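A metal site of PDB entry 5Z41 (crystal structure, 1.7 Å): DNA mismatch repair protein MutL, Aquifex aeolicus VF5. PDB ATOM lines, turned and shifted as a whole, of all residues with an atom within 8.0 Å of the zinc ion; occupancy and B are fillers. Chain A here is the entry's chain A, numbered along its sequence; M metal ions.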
ATOM      1  N   HIS A  30       8.382  29.559 -10.912  1.00  0.00           N
ATOM      2  CA  HIS A  30       8.366  29.147 -12.311  1.00  0.00           C
ATOM      3  C   HIS A  30       7.871  27.711 -12.463  1.00  0.00           C
ATOM      4  O   HIS A  30       7.027  27.414 -13.319  1.00  0.00           O
ATOM      5  CB  HIS A  30       9.749  29.313 -12.926  1.00  0.00           C
ATOM      6  CG  HIS A  30      10.318  30.694 -12.760  1.00  0.00           C
ATOM      7  ND1 HIS A  30       9.692  31.815 -13.248  1.00  0.00           N
ATOM      8  CD2 HIS A  30      11.463  31.118 -12.167  1.00  0.00           C
ATOM      9  CE1 HIS A  30      10.424  32.881 -12.963  1.00  0.00           C
ATOM     10  NE2 HIS A  30      11.498  32.493 -12.315  1.00  0.00           N
ATOM     11  N   LEU A  31       8.382  26.805 -11.633  1.00  0.00           N
ATOM     12  CA  LEU A  31       7.900  25.435 -11.667  1.00  0.00           C
ATOM     13  C   LEU A  31       6.440  25.352 -11.240  1.00  0.00           C
ATOM     14  O   LEU A  31       5.679  24.526 -11.762  1.00  0.00           O
ATOM     15  CB  LEU A  31       8.799  24.530 -10.802  1.00  0.00           C
ATOM     16  CG  LEU A  31      10.231  24.381 -11.307  1.00  0.00           C
ATOM     17  CD1 LEU A  31      11.075  23.500 -10.386  1.00  0.00           C
ATOM     18  CD2 LEU A  31      10.264  23.829 -12.742  1.00  0.00           C
ATOM     19  N   GLU A  34       4.394  26.461 -14.136  1.00  0.00           N
ATOM     20  CA  GLU A  34       4.460  25.360 -15.097  1.00  0.00           C
ATOM     21  C   GLU A  34       3.433  24.285 -14.760  1.00  0.00           C
ATOM     22  O   GLU A  34       2.681  23.827 -15.636  1.00  0.00           O
ATOM     23  CB  GLU A  34       5.865  24.783 -15.123  1.00  0.00           C
ATOM     24  CG  GLU A  34       6.023  23.536 -15.989  1.00  0.00           C
ATOM     25  CD  GLU A  34       7.436  23.008 -15.969  1.00  0.00           C
ATOM     26  OE1 GLU A  34       8.337  23.731 -15.490  1.00  0.00           O
ATOM     27  OE2 GLU A  34       7.656  21.870 -16.441  1.00  0.00           O
ATOM     28  N   ARG A  35       3.378  23.871 -13.488  1.00  0.00           N
ATOM     29  CA  ARG A  35       2.426  22.833 -13.110  1.00  0.00           C
ATOM     30  C   ARG A  35       0.982  23.326 -13.285  1.00  0.00           C
ATOM     31  O   ARG A  35       0.127  22.591 -13.779  1.00  0.00           O
ATOM     32  CB  ARG A  35       2.683  22.382 -11.679  1.00  0.00           C
ATOM     33  CG  ARG A  35       1.594  21.496 -11.080  1.00  0.00           C
ATOM     34  CD  ARG A  35       1.323  20.238 -11.912  1.00  0.00           C
ATOM     35  NE  ARG A  35       2.408  19.246 -11.825  1.00  0.00           N
ATOM     36  CZ  ARG A  35       2.293  17.991 -12.250  1.00  0.00           C
ATOM     37  NH1 ARG A  35       1.145  17.574 -12.765  1.00  0.00           N
ATOM     38  NH2 ARG A  35       3.316  17.149 -12.142  1.00  0.00           N
ATOM     39  N   LEU A  46       5.792  20.671 -23.476  1.00  0.00           N
ATOM     40  CA  LEU A  46       6.255  22.026 -23.186  1.00  0.00           C
ATOM     41  C   LEU A  46       7.605  21.984 -22.470  1.00  0.00           C
ATOM     42  O   LEU A  46       7.900  21.075 -21.695  1.00  0.00           O
ATOM     43  CB  LEU A  46       5.233  22.779 -22.338  1.00  0.00           C
ATOM     44  CG  LEU A  46       3.966  23.196 -23.092  1.00  0.00           C
ATOM     45  CD1 LEU A  46       2.829  23.448 -22.131  1.00  0.00           C
ATOM     46  CD2 LEU A  46       4.245  24.446 -23.909  1.00  0.00           C
ATOM     47  N   ALA A  47       8.436  22.981 -22.766  1.00  0.00           N
ATOM     48  CA  ALA A  47       9.764  23.051 -22.186  1.00  0.00           C
ATOM     49  C   ALA A  47       9.680  23.211 -20.667  1.00  0.00           C
ATOM     50  O   ALA A  47       8.811  23.925 -20.157  1.00  0.00           O
ATOM     51  CB  ALA A  47      10.545  24.219 -22.786  1.00  0.00           C
ATOM     52  N   CYS A  48      10.559  22.534 -19.948  1.00  0.00           N
ATOM     53  CA  CYS A  48      10.577  22.680 -18.497  1.00  0.00           C
ATOM     54  C   CYS A  48      11.087  24.077 -18.121  1.00  0.00           C
ATOM     55  O   CYS A  48      12.014  24.595 -18.749  1.00  0.00           O
ATOM     56  CB  CYS A  48      11.437  21.607 -17.847  1.00  0.00           C
ATOM     57  SG  CYS A  48      11.501  21.712 -16.036  1.00  0.00           S
ATOM     58  N   ARG A  49      10.477  24.673 -17.100  1.00  0.00           N
ATOM     59  CA  ARG A  49      10.831  26.016 -16.661  1.00  0.00           C
ATOM     60  C   ARG A  49      11.998  26.046 -15.671  1.00  0.00           C
ATOM     61  O   ARG A  49      12.331  27.129 -15.176  1.00  0.00           O
ATOM     62  CB  ARG A  49       9.605  26.718 -16.062  1.00  0.00           C
ATOM     63  CG  ARG A  49       8.355  26.724 -16.938  1.00  0.00           C
ATOM     64  CD  ARG A  49       7.542  28.007 -16.735  1.00  0.00           C
ATOM     65  NE  ARG A  49       6.403  28.057 -17.630  1.00  0.00           N
ATOM     66  CZ  ARG A  49       5.402  28.923 -17.478  1.00  0.00           C
ATOM     67  NH1 ARG A  49       5.439  29.807 -16.487  1.00  0.00           N
ATOM     68  NH2 ARG A  49       4.375  28.941 -18.306  1.00  0.00           N
ATOM     69  N   ILE A  50      12.638  24.901 -15.415  1.00  0.00           N
ATOM     70  CA  ILE A  50      13.876  24.867 -14.639  1.00  0.00           C
ATOM     71  C   ILE A  50      14.940  25.759 -15.259  1.00  0.00           C
ATOM     72  O   ILE A  50      15.882  26.193 -14.579  1.00  0.00           O
ATOM     73  CB  ILE A  50      14.393  23.414 -14.495  1.00  0.00           C
ATOM     74  CG1 ILE A  50      15.422  23.299 -13.361  1.00  0.00           C
ATOM     75  CG2 ILE A  50      15.011  22.934 -15.792  1.00  0.00           C
ATOM     76  CD1 ILE A  50      14.825  23.468 -11.999  1.00  0.00           C
ATOM     77  N   SER A  51      14.813  26.048 -16.560  1.00  0.00           N
ATOM     78  CA  SER A  51      15.789  26.874 -17.255  1.00  0.00           C
ATOM     79  C   SER A  51      15.502  28.366 -17.140  1.00  0.00           C
ATOM     80  O   SER A  51      16.402  29.170 -17.405  1.00  0.00           O
ATOM     81  CB  SER A  51      15.843  26.475 -18.731  1.00  0.00           C
ATOM     82  OG  SER A  51      14.535  26.413 -19.289  1.00  0.00           O
ATOM     83  N   VAL A  78       5.629  18.383  -7.762  1.00  0.00           N
ATOM     84  CA  VAL A  78       6.609  18.222  -8.812  1.00  0.00           C
ATOM     85  C   VAL A  78       6.024  18.787 -10.096  1.00  0.00           C
ATOM     86  O   VAL A  78       4.810  18.747 -10.305  1.00  0.00           O
ATOM     87  CB  VAL A  78       6.974  16.716  -8.871  1.00  0.00           C
ATOM     88  CG1 VAL A  78       6.220  15.990  -9.975  1.00  0.00           C
ATOM     89  CG2 VAL A  78       8.447  16.508  -8.899  1.00  0.00           C
ATOM     90  N   CYS A  79       6.885  19.362 -10.945  1.00  0.00           N
ATOM     91  CA  CYS A  79       6.456  19.790 -12.259  1.00  0.00           C
ATOM     92  C   CYS A  79       6.237  18.546 -13.121  1.00  0.00           C
ATOM     93  O   CYS A  79       6.581  17.436 -12.716  1.00  0.00           O
ATOM     94  CB  CYS A  79       7.502  20.743 -12.877  1.00  0.00           C
ATOM     95  SG  CYS A  79       8.926  19.921 -13.630  1.00  0.00           S
ATOM     96  N   PRO A  80       5.633  18.693 -14.310  1.00  0.00           N
ATOM     97  CA  PRO A  80       5.413  17.509 -15.150  1.00  0.00           C
ATOM     98  C   PRO A  80       6.672  16.744 -15.511  1.00  0.00           C
ATOM     99  O   PRO A  80       6.590  15.563 -15.863  1.00  0.00           O
ATOM    100  CB  PRO A  80       4.744  18.094 -16.402  1.00  0.00           C
ATOM    101  CG  PRO A  80       4.000  19.261 -15.875  1.00  0.00           C
ATOM    102  CD  PRO A  80       4.897  19.861 -14.818  1.00  0.00           C
ATOM    103  N   HIS A  81       7.847  17.369 -15.426  1.00  0.00           N
ATOM    104  CA  HIS A  81       9.104  16.718 -15.722  1.00  0.00           C
ATOM    105  C   HIS A  81       9.751  16.064 -14.505  1.00  0.00           C
ATOM    106  O   HIS A  81      10.755  15.366 -14.659  1.00  0.00           O
ATOM    107  CB  HIS A  81      10.056  17.725 -16.363  1.00  0.00           C
ATOM    108  CG  HIS A  81       9.472  18.412 -17.546  1.00  0.00           C
ATOM    109  ND1 HIS A  81       8.822  19.630 -17.458  1.00  0.00           N
ATOM    110  CD2 HIS A  81       9.353  18.020 -18.832  1.00  0.00           C
ATOM    111  CE1 HIS A  81       8.374  19.968 -18.652  1.00  0.00           C
ATOM    112  NE2 HIS A  81       8.680  19.007 -19.499  1.00  0.00           N
ATOM    113  N   GLY A  82       9.190  16.270 -13.320  1.00  0.00           N
ATOM    114  CA  GLY A  82       9.696  15.643 -12.129  1.00  0.00           C
ATOM    115  C   GLY A  82      10.603  16.505 -11.287  1.00  0.00           C
ATOM    116  O   GLY A  82      11.214  15.996 -10.350  1.00  0.00           O
ATOM    117  N   ARG A  83      10.696  17.797 -11.580  1.00  0.00           N
ATOM    118  CA  ARG A  83      11.482  18.695 -10.743  1.00  0.00           C
ATOM    119  C   ARG A  83      10.619  19.138  -9.565  1.00  0.00           C
ATOM    120  O   ARG A  83       9.463  19.532  -9.759  1.00  0.00           O
ATOM    121  CB  ARG A  83      11.935  19.914 -11.530  1.00  0.00           C
ATOM    122  CG  ARG A  83      12.447  19.597 -12.924  1.00  0.00           C
ATOM    123  CD  ARG A  83      13.963  19.467 -12.963  1.00  0.00           C
ATOM    124  NE  ARG A  83      14.467  18.513 -11.988  1.00  0.00           N
ATOM    125  CZ  ARG A  83      14.413  17.190 -12.129  1.00  0.00           C
ATOM    126  NH1 ARG A  83      13.859  16.665 -13.216  1.00  0.00           N
ATOM    127  NH2 ARG A  83      14.892  16.401 -11.181  1.00  0.00           N
ATOM    128  N   PRO A  84      11.137  19.087  -8.331  1.00  0.00           N
ATOM    129  CA  PRO A  84      10.315  19.479  -7.177  1.00  0.00           C
ATOM    130  C   PRO A  84       9.924  20.943  -7.294  1.00  0.00           C
ATOM    131  O   PRO A  84      10.759  21.798  -7.569  1.00  0.00           O
ATOM    132  CB  PRO A  84      11.238  19.245  -5.979  1.00  0.00           C
ATOM    133  CG  PRO A  84      12.339  18.357  -6.492  1.00  0.00           C
ATOM    134  CD  PRO A  84      12.512  18.719  -7.931  1.00  0.00           C
ATOM    135  N   ILE A  85       8.622  21.220  -7.097  1.00  0.00           N
ATOM    136  CA  ILE A  85       8.147  22.590  -7.113  1.00  0.00           C
ATOM    137  C   ILE A  85       8.665  23.368  -5.908  1.00  0.00           C
ATOM    138  O   ILE A  85       8.804  24.601  -5.956  1.00  0.00           O
ATOM    139  CB  ILE A  85       6.603  22.588  -7.178  1.00  0.00           C
ATOM    140  CG1 ILE A  85       6.153  22.118  -8.564  1.00  0.00           C
ATOM    141  CG2 ILE A  85       6.006  23.957  -6.837  1.00  0.00           C
ATOM    142  CD1 ILE A  85       4.654  21.836  -8.648  1.00  0.00           C
HETATM  143 ZN    ZN M   1       9.228  20.942 -15.706  1.00  0.00          ZN
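Of the 18 residues printed, 4 come within 4 Å of the zinc ion. The nearest printed residue that does not touch the zinc ion is Arg 49 (4.2 Å).
The zinc ion is bound by OE2 of Glu 34 (2.0 Å), ND1 of His 81 (2.2 Å), SG of Cys 79 (2.3 Å) and SG of Cys 48 (2.4 Å).
The backbone carbonyl oxygen (O) of Cys 79 is in hydrogen-bond range of the guanidinium group (NH2) of Arg 35. The backbone NH (N) of Gly 82 sits close to the side-chain sulfur (SG) of Cys 79 (3.7 Å). The side-chain sulfur of Cys 48 sits close to the backbone NH of Ile 50 (3.4 Å). N of Arg 83 lies close to SG of Cys 79 (3.4 Å). The backbone NH (N) of Arg 49 sits at hydrogen-bond distance from the side-chain carboxylate (OE1) of Glu 34, at 2.8 Å. A ring nitrogen (NE2) of His 81 sits at hydrogen-bond distance from the backbone carbonyl oxygen (O) of Leu 46, at 3.1 Å. The backbone carbonyl oxygen (O) of Cys 48 is in hydrogen-bond range of the side-chain hydroxyl (OG) of Ser 51 (3.2 Å).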
